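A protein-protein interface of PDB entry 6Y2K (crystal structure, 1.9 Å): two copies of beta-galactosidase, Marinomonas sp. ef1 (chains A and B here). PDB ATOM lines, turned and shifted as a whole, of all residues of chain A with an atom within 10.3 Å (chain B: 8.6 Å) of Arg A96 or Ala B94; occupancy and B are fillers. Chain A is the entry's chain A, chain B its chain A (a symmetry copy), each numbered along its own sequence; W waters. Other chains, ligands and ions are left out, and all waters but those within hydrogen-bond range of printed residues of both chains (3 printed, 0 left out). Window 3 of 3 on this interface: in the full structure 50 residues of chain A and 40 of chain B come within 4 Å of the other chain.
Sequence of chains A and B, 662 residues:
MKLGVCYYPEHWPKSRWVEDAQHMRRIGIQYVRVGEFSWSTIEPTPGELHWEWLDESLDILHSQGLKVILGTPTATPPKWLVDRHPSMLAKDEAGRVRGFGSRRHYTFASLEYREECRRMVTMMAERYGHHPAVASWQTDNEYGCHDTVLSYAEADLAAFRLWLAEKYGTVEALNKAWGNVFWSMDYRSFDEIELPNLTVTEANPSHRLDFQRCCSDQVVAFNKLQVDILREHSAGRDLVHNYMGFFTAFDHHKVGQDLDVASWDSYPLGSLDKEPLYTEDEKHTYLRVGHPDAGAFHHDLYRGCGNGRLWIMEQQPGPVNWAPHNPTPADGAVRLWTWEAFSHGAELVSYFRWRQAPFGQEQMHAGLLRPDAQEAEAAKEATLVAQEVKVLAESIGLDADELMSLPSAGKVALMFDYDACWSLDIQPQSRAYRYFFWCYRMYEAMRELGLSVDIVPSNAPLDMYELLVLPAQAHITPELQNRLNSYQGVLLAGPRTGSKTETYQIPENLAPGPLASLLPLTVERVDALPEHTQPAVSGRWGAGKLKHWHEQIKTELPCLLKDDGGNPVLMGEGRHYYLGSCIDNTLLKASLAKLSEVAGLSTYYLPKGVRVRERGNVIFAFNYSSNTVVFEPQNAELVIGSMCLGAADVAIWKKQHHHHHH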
ATOM      1  N   PRO A  86      -0.553 -27.138  -0.813  1.00  0.00           N
ATOM      2  CA  PRO A  86       0.017 -25.782  -0.682  1.00  0.00           C
ATOM      3  C   PRO A  86       1.423 -25.724  -0.073  1.00  0.00           C
ATOM      4  O   PRO A  86       2.195 -24.819  -0.414  1.00  0.00           O
ATOM      5  CB  PRO A  86      -0.991 -25.051   0.223  1.00  0.00           C
ATOM      6  CG  PRO A  86      -1.774 -26.131   0.899  1.00  0.00           C
ATOM      7  CD  PRO A  86      -1.821 -27.272  -0.074  1.00  0.00           C
ATOM      8  N   LEU A  89       4.782 -25.485  -2.450  1.00  0.00           N
ATOM      9  CA  LEU A  89       5.259 -24.278  -3.111  1.00  0.00           C
ATOM     10  C   LEU A  89       6.462 -23.660  -2.407  1.00  0.00           C
ATOM     11  O   LEU A  89       6.492 -23.534  -1.184  1.00  0.00           O
ATOM     12  CB  LEU A  89       4.135 -23.245  -3.252  1.00  0.00           C
ATOM     13  CG  LEU A  89       2.977 -23.643  -4.178  1.00  0.00           C
ATOM     14  CD1 LEU A  89       1.857 -22.616  -4.084  1.00  0.00           C
ATOM     15  CD2 LEU A  89       3.426 -23.796  -5.624  1.00  0.00           C
ATOM     16  N   ALA A  90       7.455 -23.279  -3.205  1.00  0.00           N
ATOM     17  CA  ALA A  90       8.629 -22.583  -2.704  1.00  0.00           C
ATOM     18  C   ALA A  90       8.295 -21.157  -2.274  1.00  0.00           C
ATOM     19  O   ALA A  90       7.268 -20.598  -2.672  1.00  0.00           O
ATOM     20  CB  ALA A  90       9.697 -22.543  -3.786  1.00  0.00           C
ATOM     21  N   LYS A  91       9.165 -20.580  -1.455  1.00  0.00           N
ATOM     22  CA  LYS A  91       9.189 -19.125  -1.262  1.00  0.00           C
ATOM     23  C   LYS A  91      10.529 -18.583  -1.702  1.00  0.00           C
ATOM     24  O   LYS A  91      11.566 -19.214  -1.474  1.00  0.00           O
ATOM     25  CB  LYS A  91       8.930 -18.747   0.187  1.00  0.00           C
ATOM     26  CG  LYS A  91       7.501 -18.969   0.595  1.00  0.00           C
ATOM     27  CD  LYS A  91       7.244 -18.546   2.020  1.00  0.00           C
ATOM     28  CE  LYS A  91       5.768 -18.716   2.331  1.00  0.00           C
ATOM     29  NZ  LYS A  91       5.495 -18.268   3.720  1.00  0.00           N
ATOM     30  N   ASP A  92      10.504 -17.410  -2.332  1.00  0.00           N
ATOM     31  CA  ASP A  92      11.728 -16.741  -2.744  1.00  0.00           C
ATOM     32  C   ASP A  92      12.450 -16.127  -1.536  1.00  0.00           C
ATOM     33  O   ASP A  92      11.963 -16.190  -0.404  1.00  0.00           O
ATOM     34  CB  ASP A  92      11.470 -15.711  -3.868  1.00  0.00           C
ATOM     35  CG  ASP A  92      10.530 -14.590  -3.471  1.00  0.00           C
ATOM     36  OD1 ASP A  92      10.441 -14.208  -2.280  1.00  0.00           O
ATOM     37  OD2 ASP A  92       9.863 -14.076  -4.397  1.00  0.00           O
ATOM     38  N   GLU A  93      13.612 -15.549  -1.798  1.00  0.00           N
ATOM     39  CA  GLU A  93      14.451 -14.941  -0.765  1.00  0.00           C
ATOM     40  C   GLU A  93      13.749 -13.799  -0.035  1.00  0.00           C
ATOM     41  O   GLU A  93      13.999 -13.567   1.148  1.00  0.00           O
ATOM     42  CB  GLU A  93      15.748 -14.449  -1.405  1.00  0.00           C
ATOM     43  CG  GLU A  93      16.795 -13.948  -0.431  1.00  0.00           C
ATOM     44  CD  GLU A  93      18.162 -13.799  -1.074  1.00  0.00           C
ATOM     45  OE1 GLU A  93      18.269 -13.865  -2.322  1.00  0.00           O
ATOM     46  OE2 GLU A  93      19.138 -13.617  -0.319  1.00  0.00           O
ATOM     47  N   ALA A  94      12.848 -13.115  -0.742  1.00  0.00           N
ATOM     48  CA  ALA A  94      12.032 -12.056  -0.154  1.00  0.00           C
ATOM     49  C   ALA A  94      10.854 -12.557   0.685  1.00  0.00           C
ATOM     50  O   ALA A  94      10.131 -11.747   1.238  1.00  0.00           O
ATOM     51  CB  ALA A  94      11.540 -11.112  -1.247  1.00  0.00           C
ATOM     52  N   GLY A  95      10.651 -13.872   0.770  1.00  0.00           N
ATOM     53  CA  GLY A  95       9.571 -14.452   1.557  1.00  0.00           C
ATOM     54  C   GLY A  95       8.238 -14.646   0.852  1.00  0.00           C
ATOM     55  O   GLY A  95       7.275 -15.031   1.503  1.00  0.00           O
ATOM     56  N   ARG A  96       8.172 -14.407  -0.463  1.00  0.00           N
ATOM     57  CA  ARG A  96       6.913 -14.550  -1.225  1.00  0.00           C
ATOM     58  C   ARG A  96       6.779 -15.912  -1.886  1.00  0.00           C
ATOM     59  O   ARG A  96       7.757 -16.475  -2.372  1.00  0.00           O
ATOM     60  CB  ARG A  96       6.802 -13.497  -2.320  1.00  0.00           C
ATOM     61  CG  ARG A  96       6.779 -12.069  -1.808  1.00  0.00           C
ATOM     62  CD  ARG A  96       8.098 -11.355  -2.012  1.00  0.00           C
ATOM     63  NE  ARG A  96       8.019 -10.374  -3.097  1.00  0.00           N
ATOM     64  CZ  ARG A  96       8.742 -10.365  -4.221  1.00  0.00           C
ATOM     65  NH1 ARG A  96       8.542  -9.391  -5.102  1.00  0.00           N
ATOM     66  NH2 ARG A  96       9.655 -11.296  -4.490  1.00  0.00           N
ATOM     67  N   VAL A  97       5.551 -16.411  -1.937  1.00  0.00           N
ATOM     68  CA  VAL A  97       5.271 -17.706  -2.549  1.00  0.00           C
ATOM     69  C   VAL A  97       5.574 -17.618  -4.050  1.00  0.00           C
ATOM     70  O   VAL A  97       5.285 -16.600  -4.693  1.00  0.00           O
ATOM     71  CB  VAL A  97       3.812 -18.158  -2.295  1.00  0.00           C
ATOM     72  CG1 VAL A  97       3.483 -19.437  -3.073  1.00  0.00           C
ATOM     73  CG2 VAL A  97       3.581 -18.372  -0.802  1.00  0.00           C
ATOM     74  N   ARG A  98       6.187 -18.675  -4.579  1.00  0.00           N
ATOM     75  CA  ARG A  98       6.481 -18.785  -6.001  1.00  0.00           C
ATOM     76  C   ARG A  98       5.396 -19.662  -6.622  1.00  0.00           C
ATOM     77  O   ARG A  98       5.425 -20.895  -6.494  1.00  0.00           O
ATOM     78  CB  ARG A  98       7.868 -19.383  -6.219  1.00  0.00           C
ATOM     79  CG  ARG A  98       8.959 -18.661  -5.451  1.00  0.00           C
ATOM     80  CD  ARG A  98      10.340 -19.031  -5.950  1.00  0.00           C
ATOM     81  NE  ARG A  98      10.644 -18.413  -7.243  1.00  0.00           N
ATOM     82  CZ  ARG A  98      11.785 -18.567  -7.909  1.00  0.00           C
ATOM     83  NH1 ARG A  98      12.762 -19.331  -7.418  1.00  0.00           N
ATOM     84  NH2 ARG A  98      11.953 -17.957  -9.081  1.00  0.00           N
ATOM     85  N   GLY A  99       4.437 -19.014  -7.283  1.00  0.00           N
ATOM     86  CA  GLY A  99       3.178 -19.661  -7.647  1.00  0.00           C
ATOM     87  C   GLY A  99       3.146 -20.375  -8.985  1.00  0.00           C
ATOM     88  O   GLY A  99       4.048 -20.233  -9.816  1.00  0.00           O
ATOM     89  N   PHE A 100       2.078 -21.145  -9.167  1.00  0.00           N
ATOM     90  CA  PHE A 100       1.663 -21.698 -10.457  1.00  0.00           C
ATOM     91  C   PHE A 100       1.442 -20.605 -11.514  1.00  0.00           C
ATOM     92  O   PHE A 100       1.097 -19.459 -11.188  1.00  0.00           O
ATOM     93  CB  PHE A 100       0.360 -22.494 -10.261  1.00  0.00           C
ATOM     94  CG  PHE A 100      -0.070 -23.294 -11.464  1.00  0.00           C
ATOM     95  CD1 PHE A 100       0.360 -24.606 -11.640  1.00  0.00           C
ATOM     96  CD2 PHE A 100      -0.924 -22.745 -12.403  1.00  0.00           C
ATOM     97  CE1 PHE A 100      -0.032 -25.346 -12.752  1.00  0.00           C
ATOM     98  CE2 PHE A 100      -1.315 -23.479 -13.524  1.00  0.00           C
ATOM     99  CZ  PHE A 100      -0.873 -24.779 -13.693  1.00  0.00           C
ATOM    100  N   THR A 107       9.193 -26.700  -4.168  1.00  0.00           N
ATOM    101  CA  THR A 107      10.468 -26.824  -3.472  1.00  0.00           C
ATOM    102  C   THR A 107      10.850 -28.299  -3.416  1.00  0.00           C
ATOM    103  O   THR A 107      10.001 -29.160  -3.154  1.00  0.00           O
ATOM    104  CB  THR A 107      10.508 -26.211  -2.059  1.00  0.00           C
ATOM    105  OG1 THR A 107      11.677 -26.697  -1.377  1.00  0.00           O
ATOM    106  CG2 THR A 107       9.257 -26.535  -1.228  1.00  0.00           C
ATOM    107  N   ASP A 147      16.393 -20.175 -10.548  1.00  0.00           N
ATOM    108  CA  ASP A 147      16.855 -20.118  -9.157  1.00  0.00           C
ATOM    109  C   ASP A 147      15.897 -20.824  -8.192  1.00  0.00           C
ATOM    110  O   ASP A 147      15.413 -20.239  -7.208  1.00  0.00           O
ATOM    111  CB  ASP A 147      17.124 -18.661  -8.742  1.00  0.00           C
ATOM    112  CG  ASP A 147      17.999 -17.926  -9.747  1.00  0.00           C
ATOM    113  OD1 ASP A 147      19.063 -18.458 -10.121  1.00  0.00           O
ATOM    114  OD2 ASP A 147      17.609 -16.824 -10.176  1.00  0.00           O
ATOM    115  N   LEU A 150      17.430 -22.954  -3.976  1.00  0.00           N
ATOM    116  CA  LEU A 150      17.185 -22.303  -2.683  1.00  0.00           C
ATOM    117  C   LEU A 150      15.718 -21.884  -2.592  1.00  0.00           C
ATOM    118  O   LEU A 150      15.181 -21.245  -3.506  1.00  0.00           O
ATOM    119  CB  LEU A 150      18.093 -21.082  -2.495  1.00  0.00           C
ATOM    120  CG  LEU A 150      19.607 -21.311  -2.505  1.00  0.00           C
ATOM    121  CD1 LEU A 150      20.331 -20.007  -2.203  1.00  0.00           C
ATOM    122  CD2 LEU A 150      20.034 -22.389  -1.518  1.00  0.00           C
ATOM    123  N   SER A 151      15.062 -22.305  -1.517  1.00  0.00           N
ATOM    124  CA  SER A 151      13.674 -21.953  -1.229  1.00  0.00           C
ATOM    125  C   SER A 151      13.563 -21.709   0.263  1.00  0.00           C
ATOM    126  O   SER A 151      14.332 -22.267   1.047  1.00  0.00           O
ATOM    127  CB  SER A 151      12.722 -23.064  -1.679  1.00  0.00           C
ATOM    128  OG  SER A 151      11.420 -22.885  -1.135  1.00  0.00           O
ATOM    129  N   TYR A 152      12.623 -20.850   0.643  1.00  0.00           N
ATOM    130  CA  TYR A 152      12.575 -20.300   1.996  1.00  0.00           C
ATOM    131  C   TYR A 152      11.193 -20.468   2.620  1.00  0.00           C
ATOM    132  O   TYR A 152      10.678 -19.564   3.291  1.00  0.00           O
ATOM    133  CB  TYR A 152      13.015 -18.834   1.949  1.00  0.00           C
ATOM    134  CG  TYR A 152      14.411 -18.665   1.377  1.00  0.00           C
ATOM    135  CD1 TYR A 152      15.532 -18.726   2.202  1.00  0.00           C
ATOM    136  CD2 TYR A 152      14.616 -18.461   0.013  1.00  0.00           C
ATOM    137  CE1 TYR A 152      16.817 -18.576   1.691  1.00  0.00           C
ATOM    138  CE2 TYR A 152      15.896 -18.313  -0.507  1.00  0.00           C
ATOM    139  CZ  TYR A 152      16.996 -18.371   0.341  1.00  0.00           C
ATOM    140  OH  TYR A 152      18.267 -18.230  -0.158  1.00  0.00           O
ATOM    141  N   ALA A 153      10.615 -21.651   2.401  1.00  0.00           N
ATOM    142  CA  ALA A 153       9.314 -22.033   2.937  1.00  0.00           C
ATOM    143  C   ALA A 153       9.503 -22.935   4.154  1.00  0.00           C
ATOM    144  O   ALA A 153      10.625 -23.367   4.456  1.00  0.00           O
ATOM    145  CB  ALA A 153       8.506 -22.752   1.867  1.00  0.00           C
ATOM    146  N   GLU A 154       8.396 -23.234   4.831  1.00  0.00           N
ATOM    147  CA  GLU A 154       8.410 -24.076   6.037  1.00  0.00           C
ATOM    148  C   GLU A 154       9.040 -25.441   5.772  1.00  0.00           C
ATOM    149  O   GLU A 154       9.819 -25.918   6.578  1.00  0.00           O
ATOM    150  CB  GLU A 154       6.996 -24.258   6.610  1.00  0.00           C
ATOM    151  CG  GLU A 154       6.954 -24.906   7.997  1.00  0.00           C
ATOM    152  CD  GLU A 154       7.561 -24.023   9.092  1.00  0.00           C
ATOM    153  OE1 GLU A 154       7.362 -22.783   9.038  1.00  0.00           O
ATOM    154  OE2 GLU A 154       8.232 -24.557  10.016  1.00  0.00           O
ATOM    155  N   ASP A 156      11.358 -26.246   3.671  1.00  0.00           N
ATOM    156  CA  ASP A 156      12.805 -26.089   3.548  1.00  0.00           C
ATOM    157  C   ASP A 156      13.469 -25.994   4.927  1.00  0.00           C
ATOM    158  O   ASP A 156      14.546 -26.545   5.142  1.00  0.00           O
ATOM    159  CB  ASP A 156      13.150 -24.840   2.731  1.00  0.00           C
ATOM    160  CG  ASP A 156      12.487 -24.835   1.364  1.00  0.00           C
ATOM    161  OD1 ASP A 156      12.928 -25.635   0.513  1.00  0.00           O
ATOM    162  OD2 ASP A 156      11.537 -24.035   1.158  1.00  0.00           O
ATOM    163  N   LEU A 195      15.841 -19.968   8.815  1.00  0.00           N
ATOM    164  CA  LEU A 195      16.383 -19.807   7.469  1.00  0.00           C
ATOM    165  C   LEU A 195      17.297 -18.570   7.461  1.00  0.00           C
ATOM    166  O   LEU A 195      17.094 -17.658   8.273  1.00  0.00           O
ATOM    167  CB  LEU A 195      15.241 -19.642   6.453  1.00  0.00           C
ATOM    168  CG  LEU A 195      14.279 -20.829   6.327  1.00  0.00           C
ATOM    169  CD1 LEU A 195      13.024 -20.430   5.560  1.00  0.00           C
ATOM    170  CD2 LEU A 195      14.983 -22.015   5.673  1.00  0.00           C
ATOM    171  N   ASN A 197      17.545 -16.153   5.235  1.00  0.00           N
ATOM    172  CA  ASN A 197      17.012 -14.961   4.563  1.00  0.00           C
ATOM    173  C   ASN A 197      16.311 -14.030   5.558  1.00  0.00           C
ATOM    174  O   ASN A 197      16.028 -14.412   6.694  1.00  0.00           O
ATOM    175  CB  ASN A 197      16.055 -15.342   3.429  1.00  0.00           C
ATOM    176  CG  ASN A 197      14.772 -15.970   3.931  1.00  0.00           C
ATOM    177  OD1 ASN A 197      14.791 -16.764   4.880  1.00  0.00           O
ATOM    178  ND2 ASN A 197      13.644 -15.614   3.303  1.00  0.00           N
ATOM    179  N   LEU A 198      16.045 -12.800   5.120  1.00  0.00           N
ATOM    180  CA  LEU A 198      15.301 -11.815   5.921  1.00  0.00           C
ATOM    181  C   LEU A 198      15.901 -11.545   7.319  1.00  0.00           C
ATOM    182  O   LEU A 198      15.183 -11.244   8.271  1.00  0.00           O
ATOM    183  CB  LEU A 198      13.819 -12.215   6.023  1.00  0.00           C
ATOM    184  CG  LEU A 198      13.067 -12.264   4.687  1.00  0.00           C
ATOM    185  CD1 LEU A 198      11.656 -12.782   4.903  1.00  0.00           C
ATOM    186  CD2 LEU A 198      13.039 -10.892   4.027  1.00  0.00           C
ATOM    187  N   LYS B  91      -3.373  -4.294  -4.179  1.00  0.00           N
ATOM    188  CA  LYS B  91      -2.031  -4.813  -3.889  1.00  0.00           C
ATOM    189  C   LYS B  91      -1.142  -4.607  -5.093  1.00  0.00           C
ATOM    190  O   LYS B  91      -1.587  -4.764  -6.234  1.00  0.00           O
ATOM    191  CB  LYS B  91      -2.066  -6.286  -3.518  1.00  0.00           C
ATOM    192  CG  LYS B  91      -2.661  -6.526  -2.159  1.00  0.00           C
ATOM    193  CD  LYS B  91      -2.647  -7.987  -1.783  1.00  0.00           C
ATOM    194  CE  LYS B  91      -3.179  -8.142  -0.369  1.00  0.00           C
ATOM    195  NZ  LYS B  91      -3.137  -9.572   0.028  1.00  0.00           N
ATOM    196  N   ASP B  92       0.117  -4.259  -4.835  1.00  0.00           N
ATOM    197  CA  ASP B  92       1.097  -4.102  -5.898  1.00  0.00           C
ATOM    198  C   ASP B  92       1.540  -5.467  -6.442  1.00  0.00           C
ATOM    199  O   ASP B  92       1.115  -6.516  -5.952  1.00  0.00           O
ATOM    200  CB  ASP B  92       2.290  -3.223  -5.456  1.00  0.00           C
ATOM    201  CG  ASP B  92       3.073  -3.792  -4.288  1.00  0.00           C
ATOM    202  OD1 ASP B  92       3.136  -5.029  -4.091  1.00  0.00           O
ATOM    203  OD2 ASP B  92       3.646  -2.960  -3.551  1.00  0.00           O
ATOM    204  N   GLU B  93       2.385  -5.429  -7.462  1.00  0.00           N
ATOM    205  CA  GLU B  93       2.887  -6.632  -8.126  1.00  0.00           C
ATOM    206  C   GLU B  93       3.658  -7.547  -7.178  1.00  0.00           C
ATOM    207  O   GLU B  93       3.650  -8.767  -7.343  1.00  0.00           O
ATOM    208  CB  GLU B  93       3.767  -6.218  -9.303  1.00  0.00           C
ATOM    209  CG  GLU B  93       4.223  -7.355 -10.195  1.00  0.00           C
ATOM    210  CD  GLU B  93       4.792  -6.866 -11.515  1.00  0.00           C
ATOM    211  OE1 GLU B  93       5.046  -5.646 -11.665  1.00  0.00           O
ATOM    212  OE2 GLU B  93       4.982  -7.712 -12.411  1.00  0.00           O
ATOM    213  N   ALA B  94       4.295  -6.949  -6.171  1.00  0.00           N
ATOM    214  CA  ALA B  94       4.998  -7.699  -5.133  1.00  0.00           C
ATOM    215  C   ALA B  94       4.087  -8.312  -4.068  1.00  0.00           C
ATOM    216  O   ALA B  94       4.581  -8.979  -3.175  1.00  0.00           O
ATOM    217  CB  ALA B  94       6.056  -6.814  -4.479  1.00  0.00           C
ATOM    218  N   GLY B  95       2.777  -8.083  -4.148  1.00  0.00           N
ATOM    219  CA  GLY B  95       1.821  -8.635  -3.196  1.00  0.00           C
ATOM    220  C   GLY B  95       1.536  -7.808  -1.954  1.00  0.00           C
ATOM    221  O   GLY B  95       0.822  -8.282  -1.079  1.00  0.00           O
ATOM    222  N   ARG B  96       2.061  -6.580  -1.871  1.00  0.00           N
ATOM    223  CA  ARG B  96       1.853  -5.715  -0.690  1.00  0.00           C
ATOM    224  C   ARG B  96       0.687  -4.755  -0.866  1.00  0.00           C
ATOM    225  O   ARG B  96       0.464  -4.228  -1.953  1.00  0.00           O
ATOM    226  CB  ARG B  96       3.090  -4.881  -0.386  1.00  0.00           C
ATOM    227  CG  ARG B  96       4.322  -5.700  -0.046  1.00  0.00           C
ATOM    228  CD  ARG B  96       5.314  -5.761  -1.189  1.00  0.00           C
ATOM    229  NE  ARG B  96       6.487  -4.923  -0.930  1.00  0.00           N
ATOM    230  CZ  ARG B  96       6.907  -3.887  -1.662  1.00  0.00           C
ATOM    231  NH1 ARG B  96       8.002  -3.236  -1.281  1.00  0.00           N
ATOM    232  NH2 ARG B  96       6.269  -3.482  -2.759  1.00  0.00           N
ATOM    233  N   VAL B  97      -0.022  -4.500   0.226  1.00  0.00           N
ATOM    234  CA  VAL B  97      -1.165  -3.593   0.209  1.00  0.00           C
ATOM    235  C   VAL B  97      -0.664  -2.177  -0.106  1.00  0.00           C
ATOM    236  O   VAL B  97       0.397  -1.761   0.376  1.00  0.00           O
ATOM    237  CB  VAL B  97      -1.948  -3.629   1.544  1.00  0.00           C
ATOM    238  CG1 VAL B  97      -3.045  -2.560   1.573  1.00  0.00           C
ATOM    239  CG2 VAL B  97      -2.550  -5.013   1.762  1.00  0.00           C
ATOM    240  N   ARG B  98      -1.421  -1.470  -0.944  1.00  0.00           N
ATOM    241  CA  ARG B  98      -1.130  -0.086  -1.290  1.00  0.00           C
ATOM    242  C   ARG B  98      -2.035   0.796  -0.432  1.00  0.00           C
ATOM    243  O   ARG B  98      -3.232   0.948  -0.720  1.00  0.00           O
ATOM    244  CB  ARG B  98      -1.367   0.158  -2.777  1.00  0.00           C
ATOM    245  CG  ARG B  98      -0.644  -0.833  -3.670  1.00  0.00           C
ATOM    246  CD  ARG B  98      -0.600  -0.366  -5.110  1.00  0.00           C
ATOM    247  NE  ARG B  98       0.355   0.727  -5.307  1.00  0.00           N
ATOM    248  CZ  ARG B  98       0.596   1.325  -6.472  1.00  0.00           C
ATOM    249  NH1 ARG B  98      -0.051   0.948  -7.577  1.00  0.00           N
ATOM    250  NH2 ARG B  98       1.486   2.313  -6.536  1.00  0.00           N
ATOM    251  N   TYR B 152      -3.430  -6.529  -7.562  1.00  0.00           N
ATOM    252  CA  TYR B 152      -3.238  -7.963  -7.365  1.00  0.00           C
ATOM    253  C   TYR B 152      -3.822  -8.429  -6.034  1.00  0.00           C
ATOM    254  O   TYR B 152      -3.226  -9.246  -5.322  1.00  0.00           O
ATOM    255  CB  TYR B 152      -1.745  -8.281  -7.483  1.00  0.00           C
ATOM    256  CG  TYR B 152      -1.168  -7.867  -8.825  1.00  0.00           C
ATOM    257  CD1 TYR B 152      -1.195  -8.739  -9.912  1.00  0.00           C
ATOM    258  CD2 TYR B 152      -0.610  -6.604  -9.016  1.00  0.00           C
ATOM    259  CE1 TYR B 152      -0.674  -8.371 -11.148  1.00  0.00           C
ATOM    260  CE2 TYR B 152      -0.089  -6.227 -10.248  1.00  0.00           C
ATOM    261  CZ  TYR B 152      -0.123  -7.119 -11.314  1.00  0.00           C
ATOM    262  OH  TYR B 152       0.384  -6.761 -12.537  1.00  0.00           O
ATOM    263  N   ASN B 197       0.937 -12.416 -11.255  1.00  0.00           N
ATOM    264  CA  ASN B 197       2.122 -11.993 -10.498  1.00  0.00           C
ATOM    265  C   ASN B 197       2.631 -13.118  -9.590  1.00  0.00           C
ATOM    266  O   ASN B 197       1.942 -14.113  -9.366  1.00  0.00           O
ATOM    267  CB  ASN B 197       1.836 -10.734  -9.672  1.00  0.00           C
ATOM    268  CG  ASN B 197       0.862 -10.985  -8.540  1.00  0.00           C
ATOM    269  OD1 ASN B 197      -0.113 -11.728  -8.704  1.00  0.00           O
ATOM    270  ND2 ASN B 197       1.123 -10.371  -7.378  1.00  0.00           N
ATOM    271  N   LEU B 198       3.850 -12.950  -9.078  1.00  0.00           N
ATOM    272  CA  LEU B 198       4.447 -13.896  -8.123  1.00  0.00           C
ATOM    273  C   LEU B 198       4.494 -15.360  -8.616  1.00  0.00           C
ATOM    274  O   LEU B 198       4.411 -16.300  -7.827  1.00  0.00           O
ATOM    275  CB  LEU B 198       3.745 -13.794  -6.758  1.00  0.00           C
ATOM    276  CG  LEU B 198       3.863 -12.430  -6.067  1.00  0.00           C
ATOM    277  CD1 LEU B 198       3.037 -12.418  -4.794  1.00  0.00           C
ATOM    278  CD2 LEU B 198       5.318 -12.097  -5.764  1.00  0.00           C
ATOM    279  N   THR B 199       4.635 -15.537  -9.921  1.00  0.00           N
ATOM    280  CA  THR B 199       4.868 -16.849 -10.503  1.00  0.00           C
ATOM    281  C   THR B 199       6.364 -17.144 -10.410  1.00  0.00           C
ATOM    282  O   THR B 199       7.167 -16.231 -10.228  1.00  0.00           O
ATOM    283  CB  THR B 199       4.414 -16.886 -11.974  1.00  0.00           C
ATOM    284  OG1 THR B 199       5.000 -15.795 -12.686  1.00  0.00           O
ATOM    285  CG2 THR B 199       2.906 -16.771 -12.073  1.00  0.00           C
ATOM    286  N   VAL B 200       6.745 -18.410 -10.543  1.00  0.00           N
ATOM    287  CA  VAL B 200       8.173 -18.795 -10.493  1.00  0.00           C
ATOM    288  C   VAL B 200       8.974 -17.985 -11.518  1.00  0.00           C
ATOM    289  O   VAL B 200      10.022 -17.408 -11.201  1.00  0.00           O
ATOM    290  CB  VAL B 200       8.375 -20.317 -10.771  1.00  0.00           C
ATOM    291  CG1 VAL B 200       9.852 -20.669 -10.929  1.00  0.00           C
ATOM    292  CG2 VAL B 200       7.762 -21.160  -9.664  1.00  0.00           C
HETATM  293  O   HOH W   1       8.952 -16.256  -8.121  1.00  0.00           O
HETATM  294  O   HOH W   2      12.704 -16.170 -11.788  1.00  0.00           O
HETATM  295  O   HOH W   3       2.233 -16.831  -5.498  1.00  0.00           O
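Arg A96 touches Ala B94, but with the chains exchanged Ala A94 does not touch Arg B96 (8.0 Å).
Val A97 touches Leu B198, but with the chains exchanged Leu A198 does not touch Val B97 (15.0 Å).
Arg A98 touches Leu B198, but with the chains exchanged Leu A198 does not touch Arg B98 (18.0 Å).
Positions printed for both chains: 91, 92, 93, 94, 95, 96, 97, 98, 152, 197 and 198.
Arg A96 touches Ala B94 (NH1 to CB, 3.6 Å).
C of Arg A98 touches O of Leu B198 (3.7 Å).
Thr B199 touches Gly A99 (CA to O, 3.5 Å).
O of Phe A100 touches CG2 of Thr B199, at 3.4 Å.
Printed residues of chain B within 4 Å of Arg A96: Ala B94 (3.6 Å).
Ala B94 touches just one residue of chain A: Arg A96 (3.6 Å).
No residue of chain B comes within 4 Å of Gly A95.
No residue of chain A comes within 4 Å of Gly B95.
No residue of chain A comes within 4 Å of Arg B96.
Printed residues of chain B within 4 Å of Arg A98: Leu B198 and Val B200.
Of the printed residues of chain B, Phe A100 touches Thr B199 (3.4 Å).
Printed residues of chain B within 4 Å of Val A97: Leu B198.
Leu A150 touches none of the printed residues of chain B.
Tyr A152 touches none of the printed residues of chain B.
Of the 24 printed residues of chain A, 5 touch a printed residue of chain B.
Hydrophobic or aromatic side chains of chain B that line the printed part of chain A: Ala B94, Leu B198 and Val B200.
The guanidinium group of Arg A96 is in salt-bridge range of the side-chain carboxylate of Asp A92 (2.8 Å).
O of Asp A147 sits at hydrogen-bond distance from NH1 of Arg A98 (2.8 Å).
The side-chain carboxylate (OD1) of Asp B92 sits at hydrogen-bond distance from the backbone NH (N) of Ala B94 (3.1 Å).
O of Ala A90 lies within hydrogen-bond range of N of Arg A98 (2.9 Å).
Water W1 lies within hydrogen-bond range of the backbone carbonyl oxygen of Thr B199, the guanidinium group of Arg A98 and the backbone carbonyl oxygen of Val B200.
Water W2 lies within hydrogen-bond range of the backbone carbonyl oxygen (O) of Val B200 and the guanidinium group (NH2) of Arg A98.
Water W3 bridges O of Val A97 (3.2 Å) and O of Leu B198 (3.2 Å).
O of Leu B198 is in hydrogen-bond range of N of Gly A99 (2.8 Å).
O of Val A97 sits close to O of Leu B198 (3.3 Å).
The backbone NH (N) of Val B200 is in hydrogen-bond range of the backbone carbonyl oxygen (O) of Gly A99, at 3.3 Å.
O of Val B200 lies within hydrogen-bond range of NH2 of Arg A98, 2.9 Å away.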
